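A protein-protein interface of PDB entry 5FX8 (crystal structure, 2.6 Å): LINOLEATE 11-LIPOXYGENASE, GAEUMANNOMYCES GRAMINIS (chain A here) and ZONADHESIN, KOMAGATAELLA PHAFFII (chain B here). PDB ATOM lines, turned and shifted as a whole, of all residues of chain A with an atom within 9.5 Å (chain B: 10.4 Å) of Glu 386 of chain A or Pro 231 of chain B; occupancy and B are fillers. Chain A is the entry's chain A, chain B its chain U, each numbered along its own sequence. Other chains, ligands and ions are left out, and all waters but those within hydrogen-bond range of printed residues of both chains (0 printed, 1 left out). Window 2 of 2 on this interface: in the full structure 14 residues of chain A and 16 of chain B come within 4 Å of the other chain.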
ATOM      1  N   ARG A 178      -1.328  -8.053  39.431  1.00  0.00           N
ATOM      2  CA  ARG A 178       0.121  -8.189  39.323  1.00  0.00           C
ATOM      3  C   ARG A 178       0.817  -7.443  40.450  1.00  0.00           C
ATOM      4  O   ARG A 178       0.380  -6.373  40.866  1.00  0.00           O
ATOM      5  CB  ARG A 178       0.601  -7.645  37.982  1.00  0.00           C
ATOM      6  CG  ARG A 178       2.051  -7.930  37.690  1.00  0.00           C
ATOM      7  CD  ARG A 178       2.575  -7.060  36.579  1.00  0.00           C
ATOM      8  NE  ARG A 178       1.934  -7.320  35.297  1.00  0.00           N
ATOM      9  CZ  ARG A 178       2.478  -7.998  34.295  1.00  0.00           C
ATOM     10  NH1 ARG A 178       3.689  -8.489  34.398  1.00  0.00           N
ATOM     11  NH2 ARG A 178       1.797  -8.178  33.185  1.00  0.00           N
ATOM     12  N   GLY A 209      11.055  -8.792  38.405  1.00  0.00           N
ATOM     13  CA  GLY A 209      10.781  -8.933  37.004  1.00  0.00           C
ATOM     14  C   GLY A 209       9.347  -8.730  36.620  1.00  0.00           C
ATOM     15  O   GLY A 209       9.009  -8.930  35.459  1.00  0.00           O
ATOM     16  N   GLY A 210       8.490  -8.334  37.554  1.00  0.00           N
ATOM     17  CA  GLY A 210       7.080  -8.169  37.263  1.00  0.00           C
ATOM     18  C   GLY A 210       6.387  -9.437  36.835  1.00  0.00           C
ATOM     19  O   GLY A 210       5.452  -9.373  36.050  1.00  0.00           O
ATOM     20  N   ARG A 211       6.830 -10.596  37.327  1.00  0.00           N
ATOM     21  CA  ARG A 211       6.256 -11.887  36.975  1.00  0.00           C
ATOM     22  C   ARG A 211       5.456 -12.527  38.111  1.00  0.00           C
ATOM     23  O   ARG A 211       5.023 -13.660  37.957  1.00  0.00           O
ATOM     24  CB  ARG A 211       7.357 -12.846  36.523  1.00  0.00           C
ATOM     25  CG  ARG A 211       8.291 -12.253  35.514  1.00  0.00           C
ATOM     26  CD  ARG A 211       9.333 -13.214  35.012  1.00  0.00           C
ATOM     27  NE  ARG A 211       8.876 -14.015  33.887  1.00  0.00           N
ATOM     28  CZ  ARG A 211       9.199 -13.810  32.613  1.00  0.00           C
ATOM     29  NH1 ARG A 211       9.984 -12.819  32.263  1.00  0.00           N
ATOM     30  NH2 ARG A 211       8.732 -14.610  31.682  1.00  0.00           N
ATOM     31  N   PHE A 213       2.057 -12.508  40.629  1.00  0.00           N
ATOM     32  CA  PHE A 213       0.667 -12.096  40.676  1.00  0.00           C
ATOM     33  C   PHE A 213       0.036 -12.653  41.943  1.00  0.00           C
ATOM     34  O   PHE A 213       0.427 -13.708  42.429  1.00  0.00           O
ATOM     35  CB  PHE A 213      -0.115 -12.600  39.470  1.00  0.00           C
ATOM     36  CG  PHE A 213       0.428 -12.168  38.163  1.00  0.00           C
ATOM     37  CD1 PHE A 213       1.516 -12.813  37.592  1.00  0.00           C
ATOM     38  CD2 PHE A 213      -0.164 -11.133  37.470  1.00  0.00           C
ATOM     39  CE1 PHE A 213       2.001 -12.411  36.378  1.00  0.00           C
ATOM     40  CE2 PHE A 213       0.326 -10.742  36.258  1.00  0.00           C
ATOM     41  CZ  PHE A 213       1.414 -11.383  35.720  1.00  0.00           C
ATOM     42  N   LEU A 240       4.344 -15.999  36.216  1.00  0.00           N
ATOM     43  CA  LEU A 240       4.517 -16.279  34.802  1.00  0.00           C
ATOM     44  C   LEU A 240       5.883 -16.931  34.605  1.00  0.00           C
ATOM     45  O   LEU A 240       6.910 -16.327  34.919  1.00  0.00           O
ATOM     46  CB  LEU A 240       4.373 -14.988  34.001  1.00  0.00           C
ATOM     47  CG  LEU A 240       4.328 -15.116  32.483  1.00  0.00           C
ATOM     48  CD1 LEU A 240       3.341 -16.173  32.045  1.00  0.00           C
ATOM     49  CD2 LEU A 240       3.954 -13.781  31.901  1.00  0.00           C
ATOM     50  N   ARG A 379      -5.997  -2.583  33.662  1.00  0.00           N
ATOM     51  CA  ARG A 379      -4.738  -1.856  33.708  1.00  0.00           C
ATOM     52  C   ARG A 379      -4.414  -1.442  35.122  1.00  0.00           C
ATOM     53  O   ARG A 379      -3.256  -1.471  35.527  1.00  0.00           O
ATOM     54  CB  ARG A 379      -4.775  -0.627  32.807  1.00  0.00           C
ATOM     55  CG  ARG A 379      -4.585  -0.922  31.361  1.00  0.00           C
ATOM     56  CD  ARG A 379      -4.412   0.352  30.582  1.00  0.00           C
ATOM     57  NE  ARG A 379      -4.453   0.107  29.152  1.00  0.00           N
ATOM     58  CZ  ARG A 379      -3.408  -0.276  28.433  1.00  0.00           C
ATOM     59  NH1 ARG A 379      -2.245  -0.445  29.021  1.00  0.00           N
ATOM     60  NH2 ARG A 379      -3.528  -0.477  27.131  1.00  0.00           N
ATOM     61  N   GLY A 382      -2.752  -4.209  36.466  1.00  0.00           N
ATOM     62  CA  GLY A 382      -1.522  -4.625  35.827  1.00  0.00           C
ATOM     63  C   GLY A 382      -1.603  -5.833  34.917  1.00  0.00           C
ATOM     64  O   GLY A 382      -0.607  -6.513  34.738  1.00  0.00           O
ATOM     65  N   LEU A 383      -2.748  -6.100  34.301  1.00  0.00           N
ATOM     66  CA  LEU A 383      -2.933  -7.299  33.496  1.00  0.00           C
ATOM     67  C   LEU A 383      -2.932  -7.071  31.979  1.00  0.00           C
ATOM     68  O   LEU A 383      -3.132  -8.034  31.242  1.00  0.00           O
ATOM     69  CB  LEU A 383      -4.236  -7.984  33.898  1.00  0.00           C
ATOM     70  CG  LEU A 383      -4.394  -8.296  35.386  1.00  0.00           C
ATOM     71  CD1 LEU A 383      -5.632  -9.046  35.642  1.00  0.00           C
ATOM     72  CD2 LEU A 383      -3.265  -9.115  35.886  1.00  0.00           C
ATOM     73  N   ILE A 384      -2.714  -5.847  31.486  1.00  0.00           N
ATOM     74  CA  ILE A 384      -2.743  -5.547  30.054  1.00  0.00           C
ATOM     75  C   ILE A 384      -1.380  -5.043  29.605  1.00  0.00           C
ATOM     76  O   ILE A 384      -0.843  -4.104  30.195  1.00  0.00           O
ATOM     77  CB  ILE A 384      -3.803  -4.491  29.714  1.00  0.00           C
ATOM     78  CG1 ILE A 384      -5.200  -5.023  29.988  1.00  0.00           C
ATOM     79  CG2 ILE A 384      -3.623  -4.023  28.269  1.00  0.00           C
ATOM     80  CD1 ILE A 384      -6.276  -4.085  29.622  1.00  0.00           C
ATOM     81  N   GLY A 385      -0.843  -5.636  28.532  1.00  0.00           N
ATOM     82  CA  GLY A 385       0.454  -5.250  27.983  1.00  0.00           C
ATOM     83  C   GLY A 385       1.663  -5.589  28.852  1.00  0.00           C
ATOM     84  O   GLY A 385       1.621  -6.424  29.728  1.00  0.00           O
ATOM     85  N   GLU A 386       2.767  -4.916  28.576  1.00  0.00           N
ATOM     86  CA  GLU A 386       3.985  -5.160  29.335  1.00  0.00           C
ATOM     87  C   GLU A 386       4.073  -4.089  30.411  1.00  0.00           C
ATOM     88  O   GLU A 386       4.604  -3.004  30.205  1.00  0.00           O
ATOM     89  CB  GLU A 386       5.199  -5.208  28.421  1.00  0.00           C
ATOM     90  CG  GLU A 386       5.261  -6.519  27.622  1.00  0.00           C
ATOM     91  CD  GLU A 386       6.444  -6.614  26.662  1.00  0.00           C
ATOM     92  OE1 GLU A 386       7.447  -5.908  26.877  1.00  0.00           O
ATOM     93  OE2 GLU A 386       6.370  -7.390  25.684  1.00  0.00           O
ATOM     94  N   ASP A 387       3.528  -4.414  31.583  1.00  0.00           N
ATOM     95  CA  ASP A 387       3.268  -3.463  32.663  1.00  0.00           C
ATOM     96  C   ASP A 387       4.224  -3.771  33.805  1.00  0.00           C
ATOM     97  O   ASP A 387       3.964  -4.652  34.629  1.00  0.00           O
ATOM     98  CB  ASP A 387       1.816  -3.556  33.122  1.00  0.00           C
ATOM     99  CG  ASP A 387       1.373  -2.354  33.935  1.00  0.00           C
ATOM    100  OD1 ASP A 387       2.142  -1.894  34.806  1.00  0.00           O
ATOM    101  OD2 ASP A 387       0.246  -1.873  33.706  1.00  0.00           O
ATOM    102  N   SER A 388       5.343  -3.055  33.832  1.00  0.00           N
ATOM    103  CA  SER A 388       6.424  -3.315  34.780  1.00  0.00           C
ATOM    104  C   SER A 388       6.783  -4.801  34.831  1.00  0.00           C
ATOM    105  O   SER A 388       7.393  -5.265  35.790  1.00  0.00           O
ATOM    106  CB  SER A 388       6.058  -2.778  36.161  1.00  0.00           C
ATOM    107  OG  SER A 388       5.613  -1.434  36.046  1.00  0.00           O
ATOM    108  N   GLY A 389       6.413  -5.540  33.782  1.00  0.00           N
ATOM    109  CA  GLY A 389       6.671  -6.954  33.656  1.00  0.00           C
ATOM    110  C   GLY A 389       6.272  -7.470  32.287  1.00  0.00           C
ATOM    111  O   GLY A 389       5.872  -6.709  31.414  1.00  0.00           O
ATOM    112  N   PRO A 390       6.372  -8.769  32.065  1.00  0.00           N
ATOM    113  CA  PRO A 390       6.030  -9.325  30.759  1.00  0.00           C
ATOM    114  C   PRO A 390       4.532  -9.427  30.540  1.00  0.00           C
ATOM    115  O   PRO A 390       3.716  -9.226  31.429  1.00  0.00           O
ATOM    116  CB  PRO A 390       6.661 -10.715  30.790  1.00  0.00           C
ATOM    117  CG  PRO A 390       6.686 -11.061  32.160  1.00  0.00           C
ATOM    118  CD  PRO A 390       6.945  -9.798  32.935  1.00  0.00           C
ATOM    119  N   ARG A 391       4.195  -9.778  29.316  1.00  0.00           N
ATOM    120  CA  ARG A 391       2.820  -9.792  28.849  1.00  0.00           C
ATOM    121  C   ARG A 391       2.263 -11.181  29.096  1.00  0.00           C
ATOM    122  O   ARG A 391       2.934 -12.173  28.823  1.00  0.00           O
ATOM    123  CB  ARG A 391       2.785  -9.427  27.362  1.00  0.00           C
ATOM    124  CG  ARG A 391       1.431  -9.175  26.736  1.00  0.00           C
ATOM    125  CD  ARG A 391       1.512  -8.904  25.215  1.00  0.00           C
ATOM    126  NE  ARG A 391       0.940  -7.603  24.900  1.00  0.00           N
ATOM    127  CZ  ARG A 391       1.673  -6.565  24.545  1.00  0.00           C
ATOM    128  NH1 ARG A 391       2.977  -6.735  24.421  1.00  0.00           N
ATOM    129  NH2 ARG A 391       1.127  -5.379  24.306  1.00  0.00           N
ATOM    130  N   LEU A 392       1.072 -11.254  29.650  1.00  0.00           N
ATOM    131  CA  LEU A 392       0.411 -12.530  29.802  1.00  0.00           C
ATOM    132  C   LEU A 392       0.147 -13.144  28.436  1.00  0.00           C
ATOM    133  O   LEU A 392      -0.548 -12.532  27.618  1.00  0.00           O
ATOM    134  CB  LEU A 392      -0.910 -12.360  30.541  1.00  0.00           C
ATOM    135  CG  LEU A 392      -0.814 -11.885  31.974  1.00  0.00           C
ATOM    136  CD1 LEU A 392      -2.183 -11.543  32.504  1.00  0.00           C
ATOM    137  CD2 LEU A 392      -0.205 -12.993  32.750  1.00  0.00           C
ATOM    138  N   PRO A 393       0.647 -14.340  28.151  1.00  0.00           N
ATOM    139  CA  PRO A 393       0.375 -14.931  26.836  1.00  0.00           C
ATOM    140  C   PRO A 393      -1.089 -15.276  26.583  1.00  0.00           C
ATOM    141  O   PRO A 393      -1.495 -15.338  25.421  1.00  0.00           O
ATOM    142  CB  PRO A 393       1.279 -16.175  26.817  1.00  0.00           C
ATOM    143  CG  PRO A 393       1.731 -16.377  28.192  1.00  0.00           C
ATOM    144  CD  PRO A 393       1.704 -15.062  28.872  1.00  0.00           C
ATOM    145  N   ASP B 191      12.268   1.331  13.330  1.00  0.00           N
ATOM    146  CA  ASP B 191      11.977   2.338  14.350  1.00  0.00           C
ATOM    147  C   ASP B 191      10.807   1.832  15.188  1.00  0.00           C
ATOM    148  O   ASP B 191       9.648   1.874  14.771  1.00  0.00           O
ATOM    149  CB  ASP B 191      11.668   3.688  13.710  1.00  0.00           C
ATOM    150  CG  ASP B 191      11.519   4.800  14.729  1.00  0.00           C
ATOM    151  OD1 ASP B 191      11.405   4.508  15.938  1.00  0.00           O
ATOM    152  OD2 ASP B 191      11.503   5.975  14.315  1.00  0.00           O
ATOM    153  N   CYS B 192      11.115   1.355  16.383  1.00  0.00           N
ATOM    154  CA  CYS B 192      10.102   0.717  17.198  1.00  0.00           C
ATOM    155  C   CYS B 192       9.141   1.717  17.783  1.00  0.00           C
ATOM    156  O   CYS B 192       8.048   1.346  18.203  1.00  0.00           O
ATOM    157  CB  CYS B 192      10.782  -0.091  18.281  1.00  0.00           C
ATOM    158  SG  CYS B 192      11.879  -1.272  17.497  1.00  0.00           S
ATOM    159  N   SER B 193       9.510   2.973  17.783  1.00  0.00           N
ATOM    160  CA  SER B 193       8.596   4.024  18.162  1.00  0.00           C
ATOM    161  C   SER B 193       7.615   4.380  17.050  1.00  0.00           C
ATOM    162  O   SER B 193       6.822   5.306  17.223  1.00  0.00           O
ATOM    163  CB  SER B 193       9.420   5.236  18.588  1.00  0.00           C
ATOM    164  OG  SER B 193       8.687   6.428  18.457  1.00  0.00           O
ATOM    165  N   GLU B 194       7.616   3.672  15.929  1.00  0.00           N
ATOM    166  CA  GLU B 194       6.829   4.100  14.779  1.00  0.00           C
ATOM    167  C   GLU B 194       6.072   2.945  14.151  1.00  0.00           C
ATOM    168  O   GLU B 194       5.911   2.884  12.938  1.00  0.00           O
ATOM    169  CB  GLU B 194       7.717   4.781  13.744  1.00  0.00           C
ATOM    170  CG  GLU B 194       8.191   6.171  14.135  1.00  0.00           C
ATOM    171  CD  GLU B 194       7.045   7.160  14.299  1.00  0.00           C
ATOM    172  OE1 GLU B 194       6.301   7.394  13.323  1.00  0.00           O
ATOM    173  OE2 GLU B 194       6.884   7.705  15.410  1.00  0.00           O
ATOM    174  N   VAL B 195       5.589   2.011  14.960  1.00  0.00           N
ATOM    175  CA  VAL B 195       4.732   0.923  14.498  1.00  0.00           C
ATOM    176  C   VAL B 195       3.297   1.300  14.829  1.00  0.00           C
ATOM    177  O   VAL B 195       3.003   1.721  15.949  1.00  0.00           O
ATOM    178  CB  VAL B 195       5.128  -0.414  15.150  1.00  0.00           C
ATOM    179  CG1 VAL B 195       4.404  -1.575  14.496  1.00  0.00           C
ATOM    180  CG2 VAL B 195       6.614  -0.632  15.065  1.00  0.00           C
ATOM    181  N   PRO B 228      -0.901   3.970  17.321  1.00  0.00           N
ATOM    182  CA  PRO B 228       0.435   3.441  17.583  1.00  0.00           C
ATOM    183  C   PRO B 228       0.373   2.143  18.375  1.00  0.00           C
ATOM    184  O   PRO B 228      -0.602   1.832  19.058  1.00  0.00           O
ATOM    185  CB  PRO B 228       1.100   4.560  18.388  1.00  0.00           C
ATOM    186  CG  PRO B 228      -0.015   5.304  19.011  1.00  0.00           C
ATOM    187  CD  PRO B 228      -1.201   5.171  18.121  1.00  0.00           C
ATOM    188  N   ILE B 229       1.441   1.373  18.264  1.00  0.00           N
ATOM    189  CA  ILE B 229       1.566   0.079  18.899  1.00  0.00           C
ATOM    190  C   ILE B 229       2.787   0.170  19.803  1.00  0.00           C
ATOM    191  O   ILE B 229       3.900   0.402  19.322  1.00  0.00           O
ATOM    192  CB  ILE B 229       1.720  -1.044  17.867  1.00  0.00           C
ATOM    193  CG1 ILE B 229       0.446  -1.252  17.061  1.00  0.00           C
ATOM    194  CG2 ILE B 229       2.128  -2.329  18.507  1.00  0.00           C
ATOM    195  CD1 ILE B 229       0.620  -2.298  16.012  1.00  0.00           C
ATOM    196  N   THR B 230       2.584   0.039  21.106  1.00  0.00           N
ATOM    197  CA  THR B 230       3.687   0.126  22.041  1.00  0.00           C
ATOM    198  C   THR B 230       3.639  -1.119  22.896  1.00  0.00           C
ATOM    199  O   THR B 230       2.732  -1.926  22.712  1.00  0.00           O
ATOM    200  CB  THR B 230       3.588   1.375  22.896  1.00  0.00           C
ATOM    201  OG1 THR B 230       2.712   1.121  23.999  1.00  0.00           O
ATOM    202  CG2 THR B 230       3.048   2.498  22.065  1.00  0.00           C
ATOM    203  N   PRO B 231       4.605  -1.351  23.784  1.00  0.00           N
ATOM    204  CA  PRO B 231       4.456  -2.468  24.728  1.00  0.00           C
ATOM    205  C   PRO B 231       3.196  -2.380  25.556  1.00  0.00           C
ATOM    206  O   PRO B 231       2.602  -3.413  25.874  1.00  0.00           O
ATOM    207  CB  PRO B 231       5.706  -2.350  25.602  1.00  0.00           C
ATOM    208  CG  PRO B 231       6.710  -1.750  24.708  1.00  0.00           C
ATOM    209  CD  PRO B 231       5.982  -0.827  23.780  1.00  0.00           C
ATOM    210  N   ALA B 232       2.754  -1.177  25.890  1.00  0.00           N
ATOM    211  CA  ALA B 232       1.629  -1.015  26.785  1.00  0.00           C
ATOM    212  C   ALA B 232       0.291  -1.237  26.108  1.00  0.00           C
ATOM    213  O   ALA B 232      -0.737  -1.160  26.783  1.00  0.00           O
ATOM    214  CB  ALA B 232       1.646   0.376  27.417  1.00  0.00           C
ATOM    215  N   SER B 233       0.252  -1.498  24.816  1.00  0.00           N
ATOM    216  CA  SER B 233      -1.034  -1.511  24.151  1.00  0.00           C
ATOM    217  C   SER B 233      -1.757  -2.834  24.389  1.00  0.00           C
ATOM    218  O   SER B 233      -1.141  -3.893  24.518  1.00  0.00           O
ATOM    219  CB  SER B 233      -0.866  -1.213  22.666  1.00  0.00           C
ATOM    220  OG  SER B 233       0.119  -2.021  22.107  1.00  0.00           O
ATOM    221  N   GLY B 234      -3.074  -2.751  24.502  1.00  0.00           N
ATOM    222  CA  GLY B 234      -3.916  -3.902  24.690  1.00  0.00           C
ATOM    223  C   GLY B 234      -4.591  -4.341  23.411  1.00  0.00           C
ATOM    224  O   GLY B 234      -4.198  -3.967  22.301  1.00  0.00           O
ATOM    225  N   LEU B 235      -5.615  -5.152  23.570  1.00  0.00           N
ATOM    226  CA  LEU B 235      -6.253  -5.749  22.431  1.00  0.00           C
ATOM    227  C   LEU B 235      -6.777  -4.670  21.495  1.00  0.00           C
ATOM    228  O   LEU B 235      -7.239  -3.637  21.955  1.00  0.00           O
ATOM    229  CB  LEU B 235      -7.346  -6.683  22.896  1.00  0.00           C
ATOM    230  CG  LEU B 235      -6.753  -7.944  23.528  1.00  0.00           C
ATOM    231  CD1 LEU B 235      -7.836  -8.748  24.189  1.00  0.00           C
ATOM    232  CD2 LEU B 235      -6.047  -8.776  22.478  1.00  0.00           C
ATOM    233  N   VAL B 237      -4.078  -5.866  19.875  1.00  0.00           N
ATOM    234  CA  VAL B 237      -2.691  -6.320  19.912  1.00  0.00           C
ATOM    235  C   VAL B 237      -2.555  -7.438  20.937  1.00  0.00           C
ATOM    236  O   VAL B 237      -2.763  -7.218  22.131  1.00  0.00           O
ATOM    237  CB  VAL B 237      -1.755  -5.153  20.244  1.00  0.00           C
ATOM    238  CG1 VAL B 237      -0.351  -5.624  20.437  1.00  0.00           C
ATOM    239  CG2 VAL B 237      -1.791  -4.167  19.156  1.00  0.00           C
ATOM    240  N   GLU B 238      -2.182  -8.633  20.481  1.00  0.00           N
ATOM    241  CA  GLU B 238      -1.873  -9.729  21.391  1.00  0.00           C
ATOM    242  C   GLU B 238      -0.406  -9.788  21.804  1.00  0.00           C
ATOM    243  O   GLU B 238      -0.103 -10.252  22.906  1.00  0.00           O
ATOM    244  CB  GLU B 238      -2.222 -11.078  20.769  1.00  0.00           C
ATOM    245  CG  GLU B 238      -3.597 -11.222  20.258  1.00  0.00           C
ATOM    246  CD  GLU B 238      -3.886 -12.657  19.874  1.00  0.00           C
ATOM    247  OE1 GLU B 238      -3.577 -13.057  18.720  1.00  0.00           O
ATOM    248  OE2 GLU B 238      -4.407 -13.394  20.742  1.00  0.00           O
ATOM    249  N   SER B 239       0.517  -9.376  20.939  1.00  0.00           N
ATOM    250  CA  SER B 239       1.938  -9.447  21.252  1.00  0.00           C
ATOM    251  C   SER B 239       2.694  -8.546  20.296  1.00  0.00           C
ATOM    252  O   SER B 239       2.247  -8.315  19.176  1.00  0.00           O
ATOM    253  CB  SER B 239       2.445 -10.873  21.139  1.00  0.00           C
ATOM    254  OG  SER B 239       2.091 -11.337  19.862  1.00  0.00           O
ATOM    255  N   PHE B 240       3.844  -8.047  20.739  1.00  0.00           N
ATOM    256  CA  PHE B 240       4.584  -7.077  19.935  1.00  0.00           C
ATOM    257  C   PHE B 240       6.053  -7.091  20.338  1.00  0.00           C
ATOM    258  O   PHE B 240       6.397  -6.625  21.424  1.00  0.00           O
ATOM    259  CB  PHE B 240       3.973  -5.691  20.101  1.00  0.00           C
ATOM    260  CG  PHE B 240       4.795  -4.591  19.541  1.00  0.00           C
ATOM    261  CD1 PHE B 240       5.124  -4.566  18.193  1.00  0.00           C
ATOM    262  CD2 PHE B 240       5.225  -3.568  20.347  1.00  0.00           C
ATOM    263  CE1 PHE B 240       5.876  -3.554  17.677  1.00  0.00           C
ATOM    264  CE2 PHE B 240       5.975  -2.554  19.832  1.00  0.00           C
ATOM    265  CZ  PHE B 240       6.300  -2.547  18.491  1.00  0.00           C
ATOM    266  N   GLU B 241       6.912  -7.618  19.469  1.00  0.00           N
ATOM    267  CA  GLU B 241       8.363  -7.523  19.616  1.00  0.00           C
ATOM    268  C   GLU B 241       8.949  -6.725  18.456  1.00  0.00           C
ATOM    269  O   GLU B 241       8.598  -6.948  17.300  1.00  0.00           O
ATOM    270  CB  GLU B 241       9.015  -8.902  19.644  1.00  0.00           C
ATOM    271  CG  GLU B 241       8.684  -9.719  20.849  1.00  0.00           C
ATOM    272  CD  GLU B 241       9.479 -11.004  20.902  1.00  0.00           C
ATOM    273  OE1 GLU B 241       9.177 -11.919  20.109  1.00  0.00           O
ATOM    274  OE2 GLU B 241      10.414 -11.098  21.727  1.00  0.00           O
ATOM    275  N   CYS B 242       9.852  -5.804  18.755  1.00  0.00           N
ATOM    276  CA  CYS B 242      10.494  -5.013  17.712  1.00  0.00           C
ATOM    277  C   CYS B 242      11.985  -4.947  18.002  1.00  0.00           C
ATOM    278  O   CYS B 242      12.405  -4.353  18.998  1.00  0.00           O
ATOM    279  CB  CYS B 242       9.892  -3.616  17.622  1.00  0.00           C
ATOM    280  SG  CYS B 242      10.654  -2.475  16.391  1.00  0.00           S
ATOM    281  N   SER B 248       7.870  -8.724  15.391  1.00  0.00           N
ATOM    282  CA  SER B 248       6.800  -9.690  15.591  1.00  0.00           C
ATOM    283  C   SER B 248       5.546  -8.974  16.065  1.00  0.00           C
ATOM    284  O   SER B 248       5.612  -8.080  16.915  1.00  0.00           O
ATOM    285  CB  SER B 248       7.183 -10.732  16.625  1.00  0.00           C
ATOM    286  OG  SER B 248       8.044 -11.690  16.086  1.00  0.00           O
ATOM    287  N   LEU B 249       4.397  -9.402  15.559  1.00  0.00           N
ATOM    288  CA  LEU B 249       3.171  -8.713  15.909  1.00  0.00           C
ATOM    289  C   LEU B 249       2.011  -9.680  15.792  1.00  0.00           C
ATOM    290  O   LEU B 249       2.014 -10.529  14.907  1.00  0.00           O
ATOM    291  CB  LEU B 249       2.989  -7.517  14.995  1.00  0.00           C
ATOM    292  CG  LEU B 249       1.872  -6.551  15.294  1.00  0.00           C
ATOM    293  CD1 LEU B 249       1.984  -6.042  16.711  1.00  0.00           C
ATOM    294  CD2 LEU B 249       1.993  -5.427  14.329  1.00  0.00           C
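Of the 19 printed residues of chain A, 5 touch a printed residue of chain B. Printed residues of chain A that touch a printed residue of chain B: Arg 379, Ile 384, Gly 385, Glu 386 and Arg 391. Hydrophobic or aromatic side chains of chain A that line the printed part of chain B: Ile 384. Of the 21 printed residues of chain B, 5 touch a printed residue of chain A. Among the printed residues, 8 pairs touch across the chains. Among the printed residues, no Asp or Glu carboxylate lies within 4 Å of a Lys or Arg side-chain nitrogen of the other chain.
The side-chain carboxylate of Glu 386 of chain A is in salt-bridge range of the guanidinium group of Arg 391 of chain A. OG1 of Thr 230 of chain B is in hydrogen-bond range of N of Ala 232 of chain B, 3.0 Å away. The side-chain hydroxyl (OG) of Ser 233 of chain B sits at hydrogen-bond distance from the backbone carbonyl oxygen (O) of Thr 230 of chain B. SG of Cys 192 of chain B forms a disulfide with SG of Cys 242 of chain B.
The guanidinium group (NH1) of Arg 379 of chain A lies within hydrogen-bond range of the backbone carbonyl oxygen (O) of Ala 232 of chain B. N of Glu 386 of chain A is in hydrogen-bond range of O of Pro 231 of chain B (3.1 Å). The guanidinium group of Arg 391 of chain A is in hydrogen-bond range of the backbone carbonyl oxygen of Pro 231 of chain B. O of Ser 233 of chain B lies within hydrogen-bond range of NH2 of Arg 391 of chain A (2.7 Å). The guanidinium group of Arg 391 of chain A lies close to the backbone carbonyl oxygen of Glu 238 of chain B, at 3.5 Å.
Glu 386 of chain A touches just one residue of chain B: Pro 231. Of chain A, only Gly 385, Glu 386 and Arg 391 come within 4 Å of Pro 231 of chain B. No residue of chain B comes within 4 Å of Asp 387 of chain A. No residue of chain A comes within 4 Å of Thr 230 of chain B. Printed residues of chain B within 4 Å of Arg 391 of chain A: Pro 231, Ser 233 and Glu 238. Of the printed residues of chain B, Ile 384 of chain A touches Gly 234. Of the printed residues of chain B, Arg 379 of chain A touches Ala 232 (2.8 Å) and Gly 234 (3.5 Å). Printed residues of chain A within 4 Å of Glu 238 of chain B: Arg 391 (3.1 Å). Printed residues of chain A within 4 Å of Gly 234 of chain B: Arg 379 and Ile 384. Val 195 of chain B touches none of the printed residues of chain A. Cys 192 of chain B touches none of the printed residues of chain A. The nearest residue of chain A that does not touch Pro 231 of chain B is Ile 384 of chain A (5.6 Å). The nearest printed residue of chain B that does not touch Arg 379 of chain A is Ser 233 of chain B (4.02 Å).
Among the printed residues, merely in contact across the chains: Arg 379 of chain A with Gly 234 of chain B, Gly 385 of chain A with Pro 231 of chain B and Ile 384 of chain A with Gly 234 of chain B.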
